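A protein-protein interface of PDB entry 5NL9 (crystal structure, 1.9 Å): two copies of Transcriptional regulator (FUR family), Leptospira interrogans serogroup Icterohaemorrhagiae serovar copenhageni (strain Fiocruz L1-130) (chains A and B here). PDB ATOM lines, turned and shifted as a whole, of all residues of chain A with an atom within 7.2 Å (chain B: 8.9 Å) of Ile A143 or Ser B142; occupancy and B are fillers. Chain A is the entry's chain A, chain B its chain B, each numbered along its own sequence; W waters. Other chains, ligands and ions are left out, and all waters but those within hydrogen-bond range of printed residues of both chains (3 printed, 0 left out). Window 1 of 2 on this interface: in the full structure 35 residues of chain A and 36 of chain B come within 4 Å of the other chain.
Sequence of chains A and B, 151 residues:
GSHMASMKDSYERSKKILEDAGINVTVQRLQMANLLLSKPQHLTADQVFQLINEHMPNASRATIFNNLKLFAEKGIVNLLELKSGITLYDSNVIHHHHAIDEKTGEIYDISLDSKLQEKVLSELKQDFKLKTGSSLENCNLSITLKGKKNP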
ATOM      1  N   LEU A  80      13.697  16.864  24.369  1.00  0.00           N
ATOM      2  CA  LEU A  80      12.361  16.817  24.963  1.00  0.00           C
ATOM      3  C   LEU A  80      12.491  16.378  26.427  1.00  0.00           C
ATOM      4  O   LEU A  80      12.893  15.247  26.689  1.00  0.00           O
ATOM      5  CB  LEU A  80      11.433  15.855  24.179  1.00  0.00           C
ATOM      6  CG  LEU A  80      10.010  15.693  24.726  1.00  0.00           C
ATOM      7  CD1 LEU A  80       9.158  16.914  24.412  1.00  0.00           C
ATOM      8  CD2 LEU A  80       9.352  14.443  24.194  1.00  0.00           C
ATOM      9  N   LYS A  83       8.325  15.654  32.764  1.00  0.00           N
ATOM     10  CA  LYS A  83       8.177  16.057  34.172  1.00  0.00           C
ATOM     11  C   LYS A  83       8.634  14.947  35.171  1.00  0.00           C
ATOM     12  O   LYS A  83       7.815  14.262  35.796  1.00  0.00           O
ATOM     13  CB  LYS A  83       6.746  16.576  34.466  1.00  0.00           C
ATOM     14  CG  LYS A  83       6.378  17.888  33.756  1.00  0.00           C
ATOM     15  CD  LYS A  83       6.741  19.144  34.568  1.00  0.00           C
ATOM     16  CE  LYS A  83       6.253  20.429  33.929  1.00  0.00           C
ATOM     17  NZ  LYS A  83       4.811  20.689  34.200  1.00  0.00           N
ATOM     18  N   HIS A  95       7.564  21.061  14.437  1.00  0.00           N
ATOM     19  CA  HIS A  95       6.839  21.445  15.654  1.00  0.00           C
ATOM     20  C   HIS A  95       5.640  20.530  15.911  1.00  0.00           C
ATOM     21  O   HIS A  95       4.800  20.353  15.034  1.00  0.00           O
ATOM     22  CB  HIS A  95       6.409  22.927  15.613  1.00  0.00           C
ATOM     23  CG  HIS A  95       5.620  23.368  16.807  1.00  0.00           C
ATOM     24  ND1 HIS A  95       6.224  23.563  18.047  1.00  0.00           N
ATOM     25  CD2 HIS A  95       4.297  23.637  16.920  1.00  0.00           C
ATOM     26  CE1 HIS A  95       5.251  23.930  18.871  1.00  0.00           C
ATOM     27  NE2 HIS A  95       4.071  23.989  18.240  1.00  0.00           N
ATOM     28  N   HIS A  96       5.606  19.910  17.100  1.00  0.00           N
ATOM     29  CA  HIS A  96       4.502  19.043  17.477  1.00  0.00           C
ATOM     30  C   HIS A  96       4.354  18.951  19.006  1.00  0.00           C
ATOM     31  O   HIS A  96       5.231  19.412  19.739  1.00  0.00           O
ATOM     32  CB  HIS A  96       4.653  17.639  16.852  1.00  0.00           C
ATOM     33  CG  HIS A  96       5.850  16.884  17.346  1.00  0.00           C
ATOM     34  ND1 HIS A  96       7.109  17.079  16.809  1.00  0.00           N
ATOM     35  CD2 HIS A  96       5.945  15.979  18.344  1.00  0.00           C
ATOM     36  CE1 HIS A  96       7.918  16.277  17.485  1.00  0.00           C
ATOM     37  NE2 HIS A  96       7.258  15.576  18.395  1.00  0.00           N
ATOM     38  N   HIS A  97       3.244  18.359  19.476  1.00  0.00           N
ATOM     39  CA  HIS A  97       2.998  18.165  20.899  1.00  0.00           C
ATOM     40  C   HIS A  97       3.018  16.680  21.210  1.00  0.00           C
ATOM     41  O   HIS A  97       3.327  15.894  20.317  1.00  0.00           O
ATOM     42  CB  HIS A  97       1.655  18.816  21.302  1.00  0.00           C
ATOM     43  CG  HIS A  97       1.622  20.265  20.917  1.00  0.00           C
ATOM     44  ND1 HIS A  97       2.513  21.171  21.472  1.00  0.00           N
ATOM     45  CD2 HIS A  97       0.911  20.885  19.951  1.00  0.00           C
ATOM     46  CE1 HIS A  97       2.258  22.326  20.878  1.00  0.00           C
ATOM     47  NE2 HIS A  97       1.295  22.200  19.960  1.00  0.00           N
ATOM     48  N   HIS A  98       2.737  16.307  22.456  1.00  0.00           N
ATOM     49  CA  HIS A  98       2.811  14.909  22.892  1.00  0.00           C
ATOM     50  C   HIS A  98       1.695  14.455  23.785  1.00  0.00           C
ATOM     51  O   HIS A  98       1.280  15.168  24.693  1.00  0.00           O
ATOM     52  CB  HIS A  98       4.123  14.696  23.681  1.00  0.00           C
ATOM     53  CG  HIS A  98       5.338  14.889  22.854  1.00  0.00           C
ATOM     54  ND1 HIS A  98       5.936  16.138  22.742  1.00  0.00           N
ATOM     55  CD2 HIS A  98       5.941  14.034  21.996  1.00  0.00           C
ATOM     56  CE1 HIS A  98       6.925  15.981  21.875  1.00  0.00           C
ATOM     57  NE2 HIS A  98       6.969  14.734  21.407  1.00  0.00           N
ATOM     58  N   ALA A  99       1.256  13.215  23.565  1.00  0.00           N
ATOM     59  CA  ALA A  99       0.306  12.532  24.428  1.00  0.00           C
ATOM     60  C   ALA A  99       1.129  11.405  25.054  1.00  0.00           C
ATOM     61  O   ALA A  99       1.938  10.753  24.376  1.00  0.00           O
ATOM     62  CB  ALA A  99      -0.853  11.965  23.629  1.00  0.00           C
ATOM     63  N   ILE A 110       1.539  14.325  18.584  1.00  0.00           N
ATOM     64  CA  ILE A 110       0.200  14.796  18.250  1.00  0.00           C
ATOM     65  C   ILE A 110       0.296  16.266  17.884  1.00  0.00           C
ATOM     66  O   ILE A 110       1.204  16.938  18.346  1.00  0.00           O
ATOM     67  CB  ILE A 110      -0.822  14.491  19.386  1.00  0.00           C
ATOM     68  CG1 ILE A 110      -2.263  14.640  18.923  1.00  0.00           C
ATOM     69  CG2 ILE A 110      -0.542  15.277  20.691  1.00  0.00           C
ATOM     70  CD1 ILE A 110      -3.249  13.930  19.857  1.00  0.00           C
ATOM     71  N   LEU A 112      -1.755  20.171  16.865  1.00  0.00           N
ATOM     72  CA  LEU A 112      -2.933  20.977  17.112  1.00  0.00           C
ATOM     73  C   LEU A 112      -3.167  21.839  15.868  1.00  0.00           C
ATOM     74  O   LEU A 112      -2.202  22.268  15.248  1.00  0.00           O
ATOM     75  CB  LEU A 112      -2.650  21.866  18.345  1.00  0.00           C
ATOM     76  CG  LEU A 112      -3.809  22.558  19.020  1.00  0.00           C
ATOM     77  CD1 LEU A 112      -4.872  21.583  19.497  1.00  0.00           C
ATOM     78  CD2 LEU A 112      -3.315  23.348  20.202  1.00  0.00           C
ATOM     79  N   GLN A 117      -4.210  26.641  17.874  1.00  0.00           N
ATOM     80  CA  GLN A 117      -2.938  26.829  18.562  1.00  0.00           C
ATOM     81  C   GLN A 117      -2.618  28.312  18.756  1.00  0.00           C
ATOM     82  O   GLN A 117      -2.161  28.707  19.837  1.00  0.00           O
ATOM     83  CB  GLN A 117      -1.823  26.144  17.761  1.00  0.00           C
ATOM     84  CG  GLN A 117      -0.510  26.066  18.497  1.00  0.00           C
ATOM     85  CD  GLN A 117       0.340  25.054  17.791  1.00  0.00           C
ATOM     86  OE1 GLN A 117       0.383  23.907  18.190  1.00  0.00           O
ATOM     87  NE2 GLN A 117       0.897  25.409  16.635  1.00  0.00           N
ATOM     88  N   VAL A 120      -4.799  29.687  21.618  1.00  0.00           N
ATOM     89  CA  VAL A 120      -4.249  29.271  22.921  1.00  0.00           C
ATOM     90  C   VAL A 120      -3.064  30.166  23.244  1.00  0.00           C
ATOM     91  O   VAL A 120      -3.002  30.706  24.351  1.00  0.00           O
ATOM     92  CB  VAL A 120      -3.865  27.768  22.927  1.00  0.00           C
ATOM     93  CG1 VAL A 120      -3.110  27.370  24.194  1.00  0.00           C
ATOM     94  CG2 VAL A 120      -5.105  26.921  22.786  1.00  0.00           C
ATOM     95  N   LEU A 124      -3.014  32.739  26.433  1.00  0.00           N
ATOM     96  CA  LEU A 124      -2.013  32.562  27.473  1.00  0.00           C
ATOM     97  C   LEU A 124      -1.117  33.783  27.594  1.00  0.00           C
ATOM     98  O   LEU A 124      -0.762  34.155  28.711  1.00  0.00           O
ATOM     99  CB  LEU A 124      -1.204  31.294  27.273  1.00  0.00           C
ATOM    100  CG  LEU A 124      -1.939  29.974  27.550  1.00  0.00           C
ATOM    101  CD1 LEU A 124      -1.131  28.843  27.089  1.00  0.00           C
ATOM    102  CD2 LEU A 124      -2.225  29.766  29.053  1.00  0.00           C
ATOM    103  N   LEU A 141       4.904  27.346  22.162  1.00  0.00           N
ATOM    104  CA  LEU A 141       3.962  26.601  22.986  1.00  0.00           C
ATOM    105  C   LEU A 141       4.292  25.113  22.954  1.00  0.00           C
ATOM    106  O   LEU A 141       4.519  24.575  21.864  1.00  0.00           O
ATOM    107  CB  LEU A 141       2.574  26.835  22.368  1.00  0.00           C
ATOM    108  CG  LEU A 141       1.392  26.480  23.192  1.00  0.00           C
ATOM    109  CD1 LEU A 141       1.201  27.505  24.275  1.00  0.00           C
ATOM    110  CD2 LEU A 141       0.144  26.451  22.322  1.00  0.00           C
ATOM    111  N   SER A 142       4.342  24.463  24.136  1.00  0.00           N
ATOM    112  CA  SER A 142       4.550  23.010  24.230  1.00  0.00           C
ATOM    113  C   SER A 142       3.436  22.430  25.069  1.00  0.00           C
ATOM    114  O   SER A 142       3.167  22.921  26.175  1.00  0.00           O
ATOM    115  CB  SER A 142       5.888  22.677  24.869  1.00  0.00           C
ATOM    116  OG  SER A 142       6.936  22.867  23.932  1.00  0.00           O
ATOM    117  N   ILE A 143       2.744  21.433  24.516  1.00  0.00           N
ATOM    118  CA  ILE A 143       1.608  20.827  25.197  1.00  0.00           C
ATOM    119  C   ILE A 143       1.886  19.352  25.398  1.00  0.00           C
ATOM    120  O   ILE A 143       2.452  18.674  24.517  1.00  0.00           O
ATOM    121  CB  ILE A 143       0.327  21.055  24.344  1.00  0.00           C
ATOM    122  CG1 ILE A 143       0.073  22.583  24.066  1.00  0.00           C
ATOM    123  CG2 ILE A 143      -0.917  20.386  24.969  1.00  0.00           C
ATOM    124  CD1 ILE A 143      -0.926  22.795  22.945  1.00  0.00           C
ATOM    125  N   THR A 144       1.491  18.870  26.568  1.00  0.00           N
ATOM    126  CA  THR A 144       1.560  17.451  26.926  1.00  0.00           C
ATOM    127  C   THR A 144       0.180  17.055  27.407  1.00  0.00           C
ATOM    128  O   THR A 144      -0.392  17.728  28.256  1.00  0.00           O
ATOM    129  CB  THR A 144       2.641  17.098  27.969  1.00  0.00           C
ATOM    130  OG1 THR A 144       2.334  17.713  29.218  1.00  0.00           O
ATOM    131  CG2 THR A 144       4.046  17.440  27.520  1.00  0.00           C
ATOM    132  N   LEU A 145      -0.348  15.989  26.853  1.00  0.00           N
ATOM    133  CA  LEU A 145      -1.644  15.446  27.263  1.00  0.00           C
ATOM    134  C   LEU A 145      -1.296  14.093  27.903  1.00  0.00           C
ATOM    135  O   LEU A 145      -0.696  13.242  27.247  1.00  0.00           O
ATOM    136  CB  LEU A 145      -2.514  15.271  26.026  1.00  0.00           C
ATOM    137  CG  LEU A 145      -3.872  14.637  26.256  1.00  0.00           C
ATOM    138  CD1 LEU A 145      -4.733  15.470  27.203  1.00  0.00           C
ATOM    139  CD2 LEU A 145      -4.560  14.413  24.914  1.00  0.00           C
ATOM    140  N   LYS A 146      -1.559  13.941  29.192  1.00  0.00           N
ATOM    141  CA  LYS A 146      -1.270  12.696  29.907  1.00  0.00           C
ATOM    142  C   LYS A 146      -2.587  12.021  30.264  1.00  0.00           C
ATOM    143  O   LYS A 146      -3.446  12.655  30.863  1.00  0.00           O
ATOM    144  CB  LYS A 146      -0.497  12.993  31.200  1.00  0.00           C
ATOM    145  CG  LYS A 146       0.949  13.387  30.974  1.00  0.00           C
ATOM    146  CD  LYS A 146       1.692  13.460  32.301  1.00  0.00           C
ATOM    147  CE  LYS A 146       3.076  14.029  32.162  1.00  0.00           C
ATOM    148  NZ  LYS A 146       3.648  14.397  33.488  1.00  0.00           N
ATOM    149  N   VAL B  93      -2.230  16.831  41.723  1.00  0.00           N
ATOM    150  CA  VAL B  93      -2.509  17.355  40.371  1.00  0.00           C
ATOM    151  C   VAL B  93      -2.215  18.861  40.345  1.00  0.00           C
ATOM    152  O   VAL B  93      -2.519  19.552  41.311  1.00  0.00           O
ATOM    153  CB  VAL B  93      -3.996  17.064  39.983  1.00  0.00           C
ATOM    154  CG1 VAL B  93      -4.324  17.536  38.558  1.00  0.00           C
ATOM    155  CG2 VAL B  93      -4.307  15.576  40.119  1.00  0.00           C
ATOM    156  N   ILE B  94      -1.629  19.356  39.235  1.00  0.00           N
ATOM    157  CA  ILE B  94      -1.304  20.778  38.998  1.00  0.00           C
ATOM    158  C   ILE B  94      -2.472  21.267  38.166  1.00  0.00           C
ATOM    159  O   ILE B  94      -2.679  20.789  37.037  1.00  0.00           O
ATOM    160  CB  ILE B  94       0.082  20.918  38.265  1.00  0.00           C
ATOM    161  CG1 ILE B  94       1.253  20.602  39.239  1.00  0.00           C
ATOM    162  CG2 ILE B  94       0.277  22.303  37.628  1.00  0.00           C
ATOM    163  CD1 ILE B  94       2.603  20.120  38.527  1.00  0.00           C
ATOM    164  N   HIS B  95      -3.265  22.171  38.732  1.00  0.00           N
ATOM    165  CA  HIS B  95      -4.485  22.619  38.050  1.00  0.00           C
ATOM    166  C   HIS B  95      -4.341  23.910  37.222  1.00  0.00           C
ATOM    167  O   HIS B  95      -5.368  24.490  36.888  1.00  0.00           O
ATOM    168  CB  HIS B  95      -5.657  22.756  39.076  1.00  0.00           C
ATOM    169  CG  HIS B  95      -5.800  21.596  40.026  1.00  0.00           C
ATOM    170  ND1 HIS B  95      -6.461  20.437  39.660  1.00  0.00           N
ATOM    171  CD2 HIS B  95      -5.343  21.457  41.296  1.00  0.00           C
ATOM    172  CE1 HIS B  95      -6.406  19.635  40.717  1.00  0.00           C
ATOM    173  NE2 HIS B  95      -5.738  20.206  41.729  1.00  0.00           N
ATOM    174  N   HIS B  96      -3.095  24.334  36.850  1.00  0.00           N
ATOM    175  CA  HIS B  96      -2.767  25.559  36.085  1.00  0.00           C
ATOM    176  C   HIS B  96      -1.633  25.264  35.073  1.00  0.00           C
ATOM    177  O   HIS B  96      -1.084  24.163  35.070  1.00  0.00           O
ATOM    178  CB  HIS B  96      -2.310  26.702  37.053  1.00  0.00           C
ATOM    179  CG  HIS B  96      -1.120  26.342  37.895  1.00  0.00           C
ATOM    180  ND1 HIS B  96      -1.260  25.642  39.087  1.00  0.00           N
ATOM    181  CD2 HIS B  96       0.197  26.543  37.663  1.00  0.00           C
ATOM    182  CE1 HIS B  96      -0.032  25.495  39.560  1.00  0.00           C
ATOM    183  NE2 HIS B  96       0.879  26.013  38.729  1.00  0.00           N
ATOM    184  N   HIS B  97      -1.296  26.238  34.219  1.00  0.00           N
ATOM    185  CA  HIS B  97      -0.225  26.091  33.215  1.00  0.00           C
ATOM    186  C   HIS B  97       0.937  26.987  33.589  1.00  0.00           C
ATOM    187  O   HIS B  97       0.902  27.625  34.645  1.00  0.00           O
ATOM    188  CB  HIS B  97      -0.744  26.366  31.789  1.00  0.00           C
ATOM    189  CG  HIS B  97      -1.909  25.499  31.468  1.00  0.00           C
ATOM    190  ND1 HIS B  97      -1.779  24.131  31.417  1.00  0.00           N
ATOM    191  CD2 HIS B  97      -3.207  25.823  31.327  1.00  0.00           C
ATOM    192  CE1 HIS B  97      -2.984  23.656  31.196  1.00  0.00           C
ATOM    193  NE2 HIS B  97      -3.888  24.637  31.126  1.00  0.00           N
ATOM    194  N   HIS B  98       1.971  27.013  32.749  1.00  0.00           N
ATOM    195  CA  HIS B  98       3.190  27.765  33.054  1.00  0.00           C
ATOM    196  C   HIS B  98       3.785  28.518  31.903  1.00  0.00           C
ATOM    197  O   HIS B  98       3.826  28.020  30.778  1.00  0.00           O
ATOM    198  CB  HIS B  98       4.265  26.799  33.576  1.00  0.00           C
ATOM    199  CG  HIS B  98       3.888  26.172  34.870  1.00  0.00           C
ATOM    200  ND1 HIS B  98       3.243  24.952  34.918  1.00  0.00           N
ATOM    201  CD2 HIS B  98       4.009  26.649  36.133  1.00  0.00           C
ATOM    202  CE1 HIS B  98       3.014  24.717  36.210  1.00  0.00           C
ATOM    203  NE2 HIS B  98       3.469  25.707  36.977  1.00  0.00           N
ATOM    204  N   LEU B 112      -5.781  29.026  31.518  1.00  0.00           N
ATOM    205  CA  LEU B 112      -6.471  29.071  30.249  1.00  0.00           C
ATOM    206  C   LEU B 112      -7.959  29.038  30.519  1.00  0.00           C
ATOM    207  O   LEU B 112      -8.404  28.353  31.450  1.00  0.00           O
ATOM    208  CB  LEU B 112      -6.039  27.840  29.425  1.00  0.00           C
ATOM    209  CG  LEU B 112      -6.345  27.822  27.914  1.00  0.00           C
ATOM    210  CD1 LEU B 112      -5.712  29.013  27.192  1.00  0.00           C
ATOM    211  CD2 LEU B 112      -5.871  26.507  27.291  1.00  0.00           C
ATOM    212  N   GLN B 117      -9.859  25.472  26.935  1.00  0.00           N
ATOM    213  CA  GLN B 117      -9.168  24.257  27.397  1.00  0.00           C
ATOM    214  C   GLN B 117      -9.937  23.009  26.949  1.00  0.00           C
ATOM    215  O   GLN B 117      -9.329  22.062  26.459  1.00  0.00           O
ATOM    216  CB  GLN B 117      -8.955  24.271  28.940  1.00  0.00           C
ATOM    217  CG  GLN B 117      -8.296  23.005  29.466  1.00  0.00           C
ATOM    218  CD  GLN B 117      -7.210  23.260  30.472  1.00  0.00           C
ATOM    219  OE1 GLN B 117      -6.579  24.312  30.501  1.00  0.00           O
ATOM    220  NE2 GLN B 117      -6.924  22.262  31.273  1.00  0.00           N
ATOM    221  N   VAL B 120      -9.357  22.369  23.230  1.00  0.00           N
ATOM    222  CA  VAL B 120      -8.039  21.767  23.015  1.00  0.00           C
ATOM    223  C   VAL B 120      -8.070  20.284  23.403  1.00  0.00           C
ATOM    224  O   VAL B 120      -7.664  19.460  22.601  1.00  0.00           O
ATOM    225  CB  VAL B 120      -6.921  22.568  23.750  1.00  0.00           C
ATOM    226  CG1 VAL B 120      -5.555  21.881  23.619  1.00  0.00           C
ATOM    227  CG2 VAL B 120      -6.841  23.981  23.191  1.00  0.00           C
ATOM    228  N   LEU B 121      -8.555  19.936  24.615  1.00  0.00           N
ATOM    229  CA  LEU B 121      -8.593  18.520  25.012  1.00  0.00           C
ATOM    230  C   LEU B 121      -9.427  17.760  24.037  1.00  0.00           C
ATOM    231  O   LEU B 121      -9.053  16.651  23.661  1.00  0.00           O
ATOM    232  CB  LEU B 121      -9.260  18.292  26.389  1.00  0.00           C
ATOM    233  CG  LEU B 121      -8.515  18.597  27.638  1.00  0.00           C
ATOM    234  CD1 LEU B 121      -9.493  18.674  28.788  1.00  0.00           C
ATOM    235  CD2 LEU B 121      -7.531  17.491  27.955  1.00  0.00           C
ATOM    236  N   LEU B 124      -7.499  17.163  20.674  1.00  0.00           N
ATOM    237  CA  LEU B 124      -6.399  16.245  20.880  1.00  0.00           C
ATOM    238  C   LEU B 124      -6.870  14.844  21.147  1.00  0.00           C
ATOM    239  O   LEU B 124      -6.288  13.907  20.602  1.00  0.00           O
ATOM    240  CB  LEU B 124      -5.471  16.724  21.995  1.00  0.00           C
ATOM    241  CG  LEU B 124      -4.672  18.002  21.718  1.00  0.00           C
ATOM    242  CD1 LEU B 124      -4.007  18.451  22.971  1.00  0.00           C
ATOM    243  CD2 LEU B 124      -3.581  17.765  20.652  1.00  0.00           C
ATOM    244  N   CYS B 139      -7.687  12.471  31.384  1.00  0.00           N
ATOM    245  CA  CYS B 139      -6.666  13.339  30.814  1.00  0.00           C
ATOM    246  C   CYS B 139      -6.377  14.537  31.617  1.00  0.00           C
ATOM    247  O   CYS B 139      -7.270  15.141  32.206  1.00  0.00           O
ATOM    248  CB  CYS B 139      -7.011  13.734  29.388  1.00  0.00           C
ATOM    249  SG  CYS B 139      -7.072  12.343  28.260  1.00  0.00           S
ATOM    250  N   ASN B 140      -5.115  14.941  31.542  1.00  0.00           N
ATOM    251  CA  ASN B 140      -4.635  16.160  32.120  1.00  0.00           C
ATOM    252  C   ASN B 140      -3.774  16.866  31.081  1.00  0.00           C
ATOM    253  O   ASN B 140      -2.858  16.269  30.522  1.00  0.00           O
ATOM    254  CB  ASN B 140      -3.827  15.860  33.371  1.00  0.00           C
ATOM    255  CG  ASN B 140      -3.679  17.111  34.167  1.00  0.00           C
ATOM    256  OD1 ASN B 140      -4.615  17.581  34.845  1.00  0.00           O
ATOM    257  ND2 ASN B 140      -2.564  17.747  33.967  1.00  0.00           N
ATOM    258  N   LEU B 141      -4.110  18.103  30.789  1.00  0.00           N
ATOM    259  CA  LEU B 141      -3.408  18.875  29.813  1.00  0.00           C
ATOM    260  C   LEU B 141      -2.431  19.755  30.543  1.00  0.00           C
ATOM    261  O   LEU B 141      -2.788  20.350  31.563  1.00  0.00           O
ATOM    262  CB  LEU B 141      -4.454  19.715  29.073  1.00  0.00           C
ATOM    263  CG  LEU B 141      -4.021  20.393  27.809  1.00  0.00           C
ATOM    264  CD1 LEU B 141      -3.861  19.383  26.683  1.00  0.00           C
ATOM    265  CD2 LEU B 141      -5.054  21.445  27.417  1.00  0.00           C
ATOM    266  N   SER B 142      -1.184  19.803  30.079  1.00  0.00           N
ATOM    267  CA  SER B 142      -0.156  20.672  30.641  1.00  0.00           C
ATOM    268  C   SER B 142       0.414  21.486  29.514  1.00  0.00           C
ATOM    269  O   SER B 142       0.912  20.932  28.537  1.00  0.00           O
ATOM    270  CB  SER B 142       0.976  19.890  31.301  1.00  0.00           C
ATOM    271  OG  SER B 142       0.559  19.390  32.557  1.00  0.00           O
ATOM    272  N   ILE B 143       0.344  22.795  29.653  1.00  0.00           N
ATOM    273  CA  ILE B 143       0.845  23.710  28.642  1.00  0.00           C
ATOM    274  C   ILE B 143       1.957  24.546  29.224  1.00  0.00           C
ATOM    275  O   ILE B 143       1.890  24.989  30.397  1.00  0.00           O
ATOM    276  CB  ILE B 143      -0.310  24.597  28.136  1.00  0.00           C
ATOM    277  CG1 ILE B 143      -1.490  23.746  27.624  1.00  0.00           C
ATOM    278  CG2 ILE B 143       0.187  25.572  27.056  1.00  0.00           C
ATOM    279  CD1 ILE B 143      -2.772  24.572  27.519  1.00  0.00           C
ATOM    280  N   THR B 144       3.000  24.708  28.427  1.00  0.00           N
ATOM    281  CA  THR B 144       4.147  25.538  28.764  1.00  0.00           C
ATOM    282  C   THR B 144       4.325  26.550  27.645  1.00  0.00           C
ATOM    283  O   THR B 144       4.390  26.185  26.470  1.00  0.00           O
ATOM    284  CB  THR B 144       5.436  24.747  29.010  1.00  0.00           C
ATOM    285  OG1 THR B 144       5.858  24.119  27.808  1.00  0.00           O
ATOM    286  CG2 THR B 144       5.329  23.755  30.160  1.00  0.00           C
ATOM    287  N   LEU B 145       4.391  27.821  28.015  1.00  0.00           N
ATOM    288  CA  LEU B 145       4.576  28.918  27.076  1.00  0.00           C
ATOM    289  C   LEU B 145       5.985  29.423  27.374  1.00  0.00           C
ATOM    290  O   LEU B 145       6.281  29.776  28.512  1.00  0.00           O
ATOM    291  CB  LEU B 145       3.518  29.987  27.370  1.00  0.00           C
ATOM    292  CG  LEU B 145       3.531  31.225  26.528  1.00  0.00           C
ATOM    293  CD1 LEU B 145       3.064  30.905  25.166  1.00  0.00           C
ATOM    294  CD2 LEU B 145       2.597  32.269  27.086  1.00  0.00           C
HETATM  295  O   HOH W   1       6.957  26.015  25.403  1.00  0.00           O
HETATM  296  O   HOH W   2       4.161  21.216  28.442  1.00  0.00           O
HETATM  297  O   HOH W   3      -0.088  16.694  31.145  1.00  0.00           O
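His A95 touches none of the printed residues of chain B. Ile A143 touches just these residues of chain B: Leu B141 (3.6 Å) and Ser B142 (3.4 Å). Of the printed residues of chain B, Thr A144 touches Asn B140 (3.7 Å), Leu B141 (3.6 Å) and Ser B142 (2.9 Å). Of the printed residues of chain B, Leu A145 touches Leu B121, Leu B124, Cys B139 and Asn B140. Of the printed residues of chain B, Lys A146 touches Cys B139 and Asn B140. Of the printed residues of chain A, Ile B143 touches Leu A124 (3.5 Å), Leu A141 (3.5 Å) and Ser A142 (3.5 Å). Of the printed residues of chain A, Leu B145 touches Leu A124 and Leu A141.
Hydrophobic or aromatic side chains of chain A that line the printed part of chain B: Ile A110, Val A120, Leu A124, Leu A141, Ile A143 and Leu A145. Along chain A the printed residues that touch a printed residue of chain B span positions 110 to 146. Of the 18 printed residues of chain B, 11 touch a printed residue of chain A. Among the printed residues, no Asp or Glu carboxylate lies within 4 Å of a Lys or Arg side-chain nitrogen of the other chain.
O of Ser A142 is in hydrogen-bond range of N of Thr B144 (2.9 Å). The backbone carbonyl oxygen of Thr A144 lies within hydrogen-bond range of the backbone NH of Ser B142 (2.9 Å). O of Lys A146 lies within hydrogen-bond range of N of Asn B140.
Water W1 bridges O of Thr B144 (2.8 Å) and N of Ser A142 (3.3 Å). Water W3 lies within hydrogen-bond range of the backbone carbonyl oxygen of Asn B140, the backbone carbonyl oxygen of Thr A144 and the side-chain hydroxyl of Ser B142. Water W2 lies within hydrogen-bond range of the backbone carbonyl oxygen of Ser A142 (3.0 Å), the backbone carbonyl oxygen of Ser B142 (3.3 Å) and the side-chain hydroxyl of Thr B144 (3.4 Å).
N of His A97 is in hydrogen-bond range of O of Ile A110, 2.7 Å away. The backbone carbonyl oxygen (O) of Ile A143 lies within hydrogen-bond range of the backbone NH (N) of His A98, 3.2 Å away. N of Leu A145 sits at hydrogen-bond distance from O of His A98, 2.8 Å away. The backbone NH of Ile B143 is in hydrogen-bond range of a ring nitrogen (ND1) of His B97, 3.1 Å away. The backbone NH of His B98 lies within hydrogen-bond range of the backbone carbonyl oxygen of Ile B143 (3.1 Å). O of His B98 is in hydrogen-bond range of N of Leu B145 (2.8 Å).
Leu A124 touches Ile B143, but with the chains exchanged Ile A143 does not touch Leu B124 (4.2 Å). Leu A124 touches Leu B145, and with the chains exchanged Leu A145 touches Leu B124. Leu A141 touches Leu B145, but with the chains exchanged Leu A145 does not touch Leu B141 (4.04 Å). Ser A142 touches Ile B143, and with the chains exchanged Ile A143 touches Ser B142. Of the 22 pairs that touch across the chains among the printed residues, 12 have their exchanged pair printed and touching as well.
Val B120 touches Val A120. Ile B143 touches Leu A124 (CG2 to CD1, 3.5 Å). Ile B143 touches Leu A141. Leu A141 touches Leu B145 (CD1 to CD1, 3.98 Å). O of Ser B142 touches O of Ser A142 (3.8 Å). Ile A143 touches Leu B141. Thr A144 touches Asn B140. CD1 of Leu A145 touches CD2 of Leu B121, at 3.5 Å. Leu A145 touches Asn B140. Lys A146 touches Cys B139.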
